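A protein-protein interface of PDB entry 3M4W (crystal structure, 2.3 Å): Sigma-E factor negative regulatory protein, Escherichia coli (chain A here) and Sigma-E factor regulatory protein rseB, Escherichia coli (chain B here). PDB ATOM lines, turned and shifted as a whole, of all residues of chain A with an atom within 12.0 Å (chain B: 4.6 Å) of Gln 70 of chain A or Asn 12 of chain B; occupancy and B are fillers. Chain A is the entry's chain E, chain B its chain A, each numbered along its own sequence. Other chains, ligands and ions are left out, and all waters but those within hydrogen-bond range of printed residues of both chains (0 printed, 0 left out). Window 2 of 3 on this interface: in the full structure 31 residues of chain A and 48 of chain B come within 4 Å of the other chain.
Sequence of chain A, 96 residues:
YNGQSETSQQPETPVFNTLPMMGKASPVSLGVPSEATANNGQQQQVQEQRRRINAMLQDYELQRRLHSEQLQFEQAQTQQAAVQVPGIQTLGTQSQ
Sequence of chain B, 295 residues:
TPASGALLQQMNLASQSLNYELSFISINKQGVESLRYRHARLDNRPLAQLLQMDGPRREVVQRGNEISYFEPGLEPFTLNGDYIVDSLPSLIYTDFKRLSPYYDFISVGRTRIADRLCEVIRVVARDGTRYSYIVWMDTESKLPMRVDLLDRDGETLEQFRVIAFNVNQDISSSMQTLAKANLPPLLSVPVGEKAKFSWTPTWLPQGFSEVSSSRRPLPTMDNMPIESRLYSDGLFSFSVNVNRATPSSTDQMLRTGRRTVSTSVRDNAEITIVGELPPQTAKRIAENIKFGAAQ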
ATOM      1  N   GLN A  63      23.954 -20.304   4.680  1.00  0.00           N
ATOM      2  CA  GLN A  63      23.644 -19.131   3.858  1.00  0.00           C
ATOM      3  C   GLN A  63      22.172 -18.731   3.956  1.00  0.00           C
ATOM      4  O   GLN A  63      21.850 -17.545   4.110  1.00  0.00           O
ATOM      5  CB  GLN A  63      23.963 -19.430   2.393  1.00  0.00           C
ATOM      6  CG  GLN A  63      24.802 -18.398   1.670  1.00  0.00           C
ATOM      7  CD  GLN A  63      26.255 -18.816   1.550  1.00  0.00           C
ATOM      8  OE1 GLN A  63      26.961 -18.378   0.641  1.00  0.00           O
ATOM      9  NE2 GLN A  63      26.711 -19.664   2.471  1.00  0.00           N
ATOM     10  N   ARG A  64      21.285 -19.721   3.843  1.00  0.00           N
ATOM     11  CA  ARG A  64      19.838 -19.492   3.913  1.00  0.00           C
ATOM     12  C   ARG A  64      19.438 -18.706   5.149  1.00  0.00           C
ATOM     13  O   ARG A  64      18.562 -17.844   5.094  1.00  0.00           O
ATOM     14  CB  ARG A  64      19.071 -20.820   3.943  1.00  0.00           C
ATOM     15  CG  ARG A  64      18.953 -21.530   2.621  1.00  0.00           C
ATOM     16  CD  ARG A  64      17.659 -22.330   2.578  1.00  0.00           C
ATOM     17  NE  ARG A  64      17.593 -23.377   3.599  1.00  0.00           N
ATOM     18  CZ  ARG A  64      16.498 -23.641   4.301  1.00  0.00           C
ATOM     19  NH1 ARG A  64      15.400 -22.927   4.085  1.00  0.00           N
ATOM     20  NH2 ARG A  64      16.498 -24.602   5.216  1.00  0.00           N
ATOM     21  N   ARG A  65      20.073 -19.036   6.265  1.00  0.00           N
ATOM     22  CA  ARG A  65      19.785 -18.399   7.543  1.00  0.00           C
ATOM     23  C   ARG A  65      20.525 -17.070   7.731  1.00  0.00           C
ATOM     24  O   ARG A  65      20.034 -16.168   8.415  1.00  0.00           O
ATOM     25  CB  ARG A  65      20.115 -19.382   8.669  1.00  0.00           C
ATOM     26  CG  ARG A  65      19.348 -20.691   8.534  1.00  0.00           C
ATOM     27  CD  ARG A  65      19.819 -21.742   9.520  1.00  0.00           C
ATOM     28  NE  ARG A  65      18.890 -22.873   9.626  1.00  0.00           N
ATOM     29  CZ  ARG A  65      18.586 -23.710   8.636  1.00  0.00           C
ATOM     30  NH1 ARG A  65      19.136 -23.562   7.436  1.00  0.00           N
ATOM     31  NH2 ARG A  65      17.730 -24.705   8.848  1.00  0.00           N
ATOM     32  N   LEU A  66      21.699 -16.940   7.124  1.00  0.00           N
ATOM     33  CA  LEU A  66      22.447 -15.695   7.236  1.00  0.00           C
ATOM     34  C   LEU A  66      21.826 -14.654   6.323  1.00  0.00           C
ATOM     35  O   LEU A  66      22.152 -13.479   6.425  1.00  0.00           O
ATOM     36  CB  LEU A  66      23.908 -15.878   6.826  1.00  0.00           C
ATOM     37  CG  LEU A  66      24.898 -16.582   7.752  1.00  0.00           C
ATOM     38  CD1 LEU A  66      26.258 -16.565   7.080  1.00  0.00           C
ATOM     39  CD2 LEU A  66      24.978 -15.880   9.100  1.00  0.00           C
ATOM     40  N   HIS A  67      20.925 -15.087   5.442  1.00  0.00           N
ATOM     41  CA  HIS A  67      20.299 -14.175   4.489  1.00  0.00           C
ATOM     42  C   HIS A  67      18.774 -14.190   4.456  1.00  0.00           C
ATOM     43  O   HIS A  67      18.169 -13.896   3.426  1.00  0.00           O
ATOM     44  CB  HIS A  67      20.840 -14.463   3.081  1.00  0.00           C
ATOM     45  CG  HIS A  67      22.304 -14.180   2.929  1.00  0.00           C
ATOM     46  ND1 HIS A  67      22.787 -12.960   2.509  1.00  0.00           N
ATOM     47  CD2 HIS A  67      23.391 -14.936   3.216  1.00  0.00           C
ATOM     48  CE1 HIS A  67      24.107 -12.972   2.548  1.00  0.00           C
ATOM     49  NE2 HIS A  67      24.498 -14.160   2.975  1.00  0.00           N
ATOM     50  N   SER A  68      18.147 -14.523   5.576  1.00  0.00           N
ATOM     51  CA  SER A  68      16.692 -14.551   5.624  1.00  0.00           C
ATOM     52  C   SER A  68      16.138 -13.131   5.776  1.00  0.00           C
ATOM     53  O   SER A  68      15.802 -12.699   6.879  1.00  0.00           O
ATOM     54  CB  SER A  68      16.232 -15.443   6.780  1.00  0.00           C
ATOM     55  OG  SER A  68      17.081 -15.296   7.906  1.00  0.00           O
ATOM     56  N   GLU A  69      16.051 -12.414   4.656  1.00  0.00           N
ATOM     57  CA  GLU A  69      15.556 -11.038   4.646  1.00  0.00           C
ATOM     58  C   GLU A  69      14.065 -10.922   4.362  1.00  0.00           C
ATOM     59  O   GLU A  69      13.660 -10.369   3.334  1.00  0.00           O
ATOM     60  CB  GLU A  69      16.318 -10.197   3.613  1.00  0.00           C
ATOM     61  CG  GLU A  69      17.584  -9.530   4.134  1.00  0.00           C
ATOM     62  CD  GLU A  69      18.641 -10.524   4.569  1.00  0.00           C
ATOM     63  OE1 GLU A  69      19.069 -11.343   3.726  1.00  0.00           O
ATOM     64  OE2 GLU A  69      19.044 -10.487   5.751  1.00  0.00           O
ATOM     65  N   GLN A  70      13.249 -11.440   5.273  1.00  0.00           N
ATOM     66  CA  GLN A  70      11.801 -11.372   5.119  1.00  0.00           C
ATOM     67  C   GLN A  70      11.331 -10.008   5.626  1.00  0.00           C
ATOM     68  O   GLN A  70      12.189  -9.271   6.159  1.00  0.00           O
ATOM     69  CB  GLN A  70      11.145 -12.502   5.917  1.00  0.00           C
ATOM     70  CG  GLN A  70       9.628 -12.583   5.808  1.00  0.00           C
ATOM     71  CD  GLN A  70       8.927 -12.159   7.084  1.00  0.00           C
ATOM     72  OE1 GLN A  70       7.723 -12.374   7.239  1.00  0.00           O
ATOM     73  NE2 GLN A  70       9.676 -11.550   8.003  1.00  0.00           N
ATOM     74  N   LEU B   8      -3.159 -14.968   1.193  1.00  0.00           N
ATOM     75  CA  LEU B   8      -1.789 -15.323   1.506  1.00  0.00           C
ATOM     76  C   LEU B   8      -1.060 -14.206   2.243  1.00  0.00           C
ATOM     77  O   LEU B   8      -0.236 -14.470   3.130  1.00  0.00           O
ATOM     78  CB  LEU B   8      -1.056 -15.708   0.218  1.00  0.00           C
ATOM     79  CG  LEU B   8      -1.611 -16.995  -0.407  1.00  0.00           C
ATOM     80  CD1 LEU B   8      -1.041 -17.228  -1.792  1.00  0.00           C
ATOM     81  CD2 LEU B   8      -1.286 -18.161   0.507  1.00  0.00           C
ATOM     82  N   GLN B   9      -1.351 -12.956   1.892  1.00  0.00           N
ATOM     83  CA  GLN B   9      -0.713 -11.844   2.585  1.00  0.00           C
ATOM     84  C   GLN B   9      -1.233 -11.832   4.013  1.00  0.00           C
ATOM     85  O   GLN B   9      -0.479 -11.593   4.967  1.00  0.00           O
ATOM     86  CB  GLN B   9      -1.027 -10.517   1.890  1.00  0.00           C
ATOM     87  CG  GLN B   9      -0.161 -10.262   0.661  1.00  0.00           C
ATOM     88  CD  GLN B   9      -0.792  -9.307  -0.329  1.00  0.00           C
ATOM     89  OE1 GLN B   9      -0.291  -9.130  -1.442  1.00  0.00           O
ATOM     90  NE2 GLN B   9      -1.899  -8.686   0.065  1.00  0.00           N
ATOM     91  N   GLN B  10      -2.529 -12.094   4.162  1.00  0.00           N
ATOM     92  CA  GLN B  10      -3.131 -12.128   5.490  1.00  0.00           C
ATOM     93  C   GLN B  10      -2.483 -13.237   6.327  1.00  0.00           C
ATOM     94  O   GLN B  10      -2.090 -12.999   7.467  1.00  0.00           O
ATOM     95  CB  GLN B  10      -4.640 -12.364   5.396  1.00  0.00           C
ATOM     96  CG  GLN B  10      -5.454 -11.120   5.057  1.00  0.00           C
ATOM     97  CD  GLN B  10      -6.948 -11.399   5.078  1.00  0.00           C
ATOM     98  OE1 GLN B  10      -7.464 -12.126   4.231  1.00  0.00           O
ATOM     99  NE2 GLN B  10      -7.644 -10.837   6.058  1.00  0.00           N
ATOM    100  N   MET B  11      -2.380 -14.438   5.757  1.00  0.00           N
ATOM    101  CA  MET B  11      -1.762 -15.577   6.448  1.00  0.00           C
ATOM    102  C   MET B  11      -0.363 -15.213   6.920  1.00  0.00           C
ATOM    103  O   MET B  11       0.035 -15.540   8.036  1.00  0.00           O
ATOM    104  CB  MET B  11      -1.668 -16.798   5.527  1.00  0.00           C
ATOM    105  CG  MET B  11      -0.838 -17.955   6.118  1.00  0.00           C
ATOM    106  SD  MET B  11      -0.632 -19.351   5.017  1.00  0.00           S
ATOM    107  CE  MET B  11       0.476 -18.557   3.824  1.00  0.00           C
ATOM    108  N   ASN B  12       0.384 -14.534   6.061  1.00  0.00           N
ATOM    109  CA  ASN B  12       1.732 -14.136   6.420  1.00  0.00           C
ATOM    110  C   ASN B  12       1.719 -13.121   7.561  1.00  0.00           C
ATOM    111  O   ASN B  12       2.511 -13.220   8.501  1.00  0.00           O
ATOM    112  CB  ASN B  12       2.470 -13.547   5.205  1.00  0.00           C
ATOM    113  CG  ASN B  12       3.711 -12.762   5.610  1.00  0.00           C
ATOM    114  OD1 ASN B  12       3.615 -11.633   6.103  1.00  0.00           O
ATOM    115  ND2 ASN B  12       4.878 -13.364   5.428  1.00  0.00           N
ATOM    116  N   LEU B  13       0.816 -12.148   7.467  1.00  0.00           N
ATOM    117  CA  LEU B  13       0.679 -11.097   8.473  1.00  0.00           C
ATOM    118  C   LEU B  13       0.273 -11.687   9.824  1.00  0.00           C
ATOM    119  O   LEU B  13       0.825 -11.333  10.876  1.00  0.00           O
ATOM    120  CB  LEU B  13      -0.353 -10.064   7.991  1.00  0.00           C
ATOM    121  CG  LEU B  13      -0.683  -8.814   8.821  1.00  0.00           C
ATOM    122  CD1 LEU B  13       0.517  -8.373   9.641  1.00  0.00           C
ATOM    123  CD2 LEU B  13      -1.128  -7.691   7.878  1.00  0.00           C
ATOM    124  N   ALA B  14      -0.686 -12.599   9.802  1.00  0.00           N
ATOM    125  CA  ALA B  14      -1.128 -13.235  11.037  1.00  0.00           C
ATOM    126  C   ALA B  14       0.055 -13.923  11.722  1.00  0.00           C
ATOM    127  O   ALA B  14       0.199 -13.862  12.945  1.00  0.00           O
ATOM    128  CB  ALA B  14      -2.221 -14.250  10.736  1.00  0.00           C
ATOM    129  N   SER B  15       0.902 -14.568  10.922  1.00  0.00           N
ATOM    130  CA  SER B  15       2.067 -15.288  11.435  1.00  0.00           C
ATOM    131  C   SER B  15       3.069 -14.409  12.147  1.00  0.00           C
ATOM    132  O   SER B  15       3.786 -14.878  13.023  1.00  0.00           O
ATOM    133  CB  SER B  15       2.780 -16.035  10.301  1.00  0.00           C
ATOM    134  OG  SER B  15       1.974 -17.097   9.821  1.00  0.00           O
ATOM    135  N   GLN B  16       3.130 -13.139  11.772  1.00  0.00           N
ATOM    136  CA  GLN B  16       4.071 -12.218  12.400  1.00  0.00           C
ATOM    137  C   GLN B  16       3.415 -11.328  13.437  1.00  0.00           C
ATOM    138  O   GLN B  16       4.109 -10.687  14.222  1.00  0.00           O
ATOM    139  CB  GLN B  16       4.710 -11.315  11.349  1.00  0.00           C
ATOM    140  CG  GLN B  16       5.399 -12.047  10.233  1.00  0.00           C
ATOM    141  CD  GLN B  16       6.749 -11.430   9.904  1.00  0.00           C
ATOM    142  OE1 GLN B  16       6.882 -10.196   9.819  1.00  0.00           O
ATOM    143  NE2 GLN B  16       7.764 -12.285   9.717  1.00  0.00           N
ATOM    144  N   ASP B  82      15.586 -12.658  10.475  1.00  0.00           N
ATOM    145  CA  ASP B  82      14.256 -12.113  10.749  1.00  0.00           C
ATOM    146  C   ASP B  82      13.246 -13.143  11.222  1.00  0.00           C
ATOM    147  O   ASP B  82      12.087 -12.811  11.492  1.00  0.00           O
ATOM    148  CB  ASP B  82      13.703 -11.385   9.517  1.00  0.00           C
ATOM    149  CG  ASP B  82      14.482 -10.118   9.191  1.00  0.00           C
ATOM    150  OD1 ASP B  82      15.008  -9.491  10.139  1.00  0.00           O
ATOM    151  OD2 ASP B  82      14.557  -9.744   7.996  1.00  0.00           O
ATOM    152  N   TYR B  83      13.689 -14.388  11.338  1.00  0.00           N
ATOM    153  CA  TYR B  83      12.819 -15.463  11.792  1.00  0.00           C
ATOM    154  C   TYR B  83      13.614 -16.754  11.817  1.00  0.00           C
ATOM    155  O   TYR B  83      14.737 -16.808  11.308  1.00  0.00           O
ATOM    156  CB  TYR B  83      11.620 -15.591  10.850  1.00  0.00           C
ATOM    157  CG  TYR B  83      12.012 -15.875   9.424  1.00  0.00           C
ATOM    158  CD1 TYR B  83      12.057 -17.177   8.942  1.00  0.00           C
ATOM    159  CD2 TYR B  83      12.354 -14.841   8.556  1.00  0.00           C
ATOM    160  CE1 TYR B  83      12.426 -17.447   7.638  1.00  0.00           C
ATOM    161  CE2 TYR B  83      12.730 -15.104   7.243  1.00  0.00           C
ATOM    162  CZ  TYR B  83      12.760 -16.408   6.797  1.00  0.00           C
ATOM    163  OH  TYR B  83      13.130 -16.683   5.513  1.00  0.00           O
ATOM    164  N   ILE B  92       5.287 -19.560   4.408  1.00  0.00           N
ATOM    165  CA  ILE B  92       4.641 -18.722   5.407  1.00  0.00           C
ATOM    166  C   ILE B  92       5.378 -17.410   5.687  1.00  0.00           C
ATOM    167  O   ILE B  92       4.760 -16.429   6.098  1.00  0.00           O
ATOM    168  CB  ILE B  92       4.452 -19.544   6.688  1.00  0.00           C
ATOM    169  CG1 ILE B  92       3.522 -20.727   6.365  1.00  0.00           C
ATOM    170  CG2 ILE B  92       3.882 -18.692   7.806  1.00  0.00           C
ATOM    171  CD1 ILE B  92       3.861 -21.994   7.136  1.00  0.00           C
ATOM    172  N   TYR B  93       6.691 -17.394   5.455  1.00  0.00           N
ATOM    173  CA  TYR B  93       7.512 -16.201   5.656  1.00  0.00           C
ATOM    174  C   TYR B  93       7.709 -15.459   4.340  1.00  0.00           C
ATOM    175  O   TYR B  93       8.583 -14.614   4.215  1.00  0.00           O
ATOM    176  CB  TYR B  93       8.883 -16.592   6.203  1.00  0.00           C
ATOM    177  CG  TYR B  93       8.823 -17.144   7.596  1.00  0.00           C
ATOM    178  CD1 TYR B  93       9.162 -18.472   7.848  1.00  0.00           C
ATOM    179  CD2 TYR B  93       8.381 -16.352   8.666  1.00  0.00           C
ATOM    180  CE1 TYR B  93       9.062 -19.009   9.128  1.00  0.00           C
ATOM    181  CE2 TYR B  93       8.275 -16.881   9.963  1.00  0.00           C
ATOM    182  CZ  TYR B  93       8.616 -18.211  10.183  1.00  0.00           C
ATOM    183  OH  TYR B  93       8.516 -18.763  11.443  1.00  0.00           O
ATOM    184  N   THR B  94       6.877 -15.782   3.365  1.00  0.00           N
ATOM    185  CA  THR B  94       6.968 -15.199   2.042  1.00  0.00           C
ATOM    186  C   THR B  94       6.162 -13.921   1.880  1.00  0.00           C
ATOM    187  O   THR B  94       5.046 -13.797   2.419  1.00  0.00           O
ATOM    188  CB  THR B  94       6.444 -16.196   0.982  1.00  0.00           C
ATOM    189  OG1 THR B  94       7.140 -17.441   1.100  1.00  0.00           O
ATOM    190  CG2 THR B  94       6.610 -15.628  -0.409  1.00  0.00           C
ATOM    191  N   PHE B  96       4.130 -12.366  -0.463  1.00  0.00           N
ATOM    192  CA  PHE B  96       3.416 -12.676  -1.680  1.00  0.00           C
ATOM    193  C   PHE B  96       3.325 -11.565  -2.710  1.00  0.00           C
ATOM    194  O   PHE B  96       3.175 -11.842  -3.891  1.00  0.00           O
ATOM    195  CB  PHE B  96       2.050 -13.243  -1.315  1.00  0.00           C
ATOM    196  CG  PHE B  96       2.145 -14.579  -0.628  1.00  0.00           C
ATOM    197  CD1 PHE B  96       2.485 -15.716  -1.354  1.00  0.00           C
ATOM    198  CD2 PHE B  96       1.976 -14.691   0.754  1.00  0.00           C
ATOM    199  CE1 PHE B  96       2.667 -16.951  -0.716  1.00  0.00           C
ATOM    200  CE2 PHE B  96       2.156 -15.921   1.407  1.00  0.00           C
ATOM    201  CZ  PHE B  96       2.500 -17.051   0.669  1.00  0.00           C
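Of the 8 printed residues of chain A, 3 touch a printed residue of chain B.
Along chain A the printed residues that touch a printed residue of chain B span positions 68 to 70.
Of the 15 printed residues of chain B, 5 touch a printed residue of chain A.
Hydrophobic or aromatic side chains of chain B that line the printed part of chain A: Tyr 83.
Among the printed residues, 8 pairs touch across the chains.
Of chain B, only Asn 12 (3.5 Å), Gln 16 (2.5 Å), Asp 82 (3.0 Å), Tyr 83 (3.3 Å) and Tyr 93 (2.8 Å) come within 4 Å of Gln 70 of chain A.
Of chain A, only Gln 70 comes within 4 Å of Asn 12 of chain B.
Leu 13 of chain B touches none of the printed residues of chain A.
No residue of chain A comes within 4 Å of Ala 14 of chain B.
Asp 82 of chain B touches three residues of chain A.
Of the printed residues of chain A, Tyr 83 of chain B touches Ser 68 (3.5 Å) and Gln 70 (3.3 Å).
No residue of chain A comes within 4 Å of Thr 94 of chain B.
Of the printed residues of chain B, Ser 68 of chain A touches Asp 82 (3.4 Å) and Tyr 83 (3.5 Å).
Printed residues of chain B within 4 Å of Glu 69 of chain A: Asp 82 (3.7 Å).
Gln 10 of chain B touches none of the printed residues of chain A.
Arg 64 of chain A touches none of the printed residues of chain B.
The nearest printed residue of chain B that does not touch Gln 70 of chain A is Thr 94 of chain B (4.9 Å).
The nearest residue of chain A that does not touch Asn 12 of chain B is Glu 69 of chain A (9.5 Å).
The nearest printed residue of chain B that does not touch Glu 69 of chain A is Tyr 83 of chain B (5.0 Å).
CE2 of Tyr 83 of chain B touches CB of Ser 68 of chain A, 3.5 Å away.
Asp 82 of chain B touches Glu 69 of chain A.
Gln 70 of chain A touches Asn 12 of chain B (OE1 to ND2, 3.5 Å).
CB of Gln 70 of chain A touches CE2 of Tyr 83 of chain B, 3.3 Å away.
Gln 70 of chain A touches Tyr 93 of chain B (CG to O, 2.8 Å).
NE2 of Gln 16 of chain B is in hydrogen-bond range of OE1 of Gln 70 of chain A (2.5 Å).
OD2 of Asp 82 of chain B lies within hydrogen-bond range of N of Gln 70 of chain A (3.5 Å).
The backbone carbonyl oxygen (O) of Ser 68 of chain A lies close to the side-chain carboxylate (OD2) of Asp 82 of chain B, at 3.4 Å.
O of Ile 92 of chain B lies within hydrogen-bond range of ND2 of Asn 12 of chain B, at 3.1 Å.
The side-chain amide nitrogen (ND2) of Asn 12 of chain B lies within hydrogen-bond range of the backbone carbonyl oxygen (O) of Thr 94 of chain B.
The backbone carbonyl oxygen (O) of Arg 65 of chain A is in hydrogen-bond range of the side-chain hydroxyl (OG) of Ser 68 of chain A (3.1 Å).
The backbone carbonyl oxygen (O) of His 67 of chain A sits close to the side-chain carboxylate (OE1) of Glu 69 of chain A (2.7 Å).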
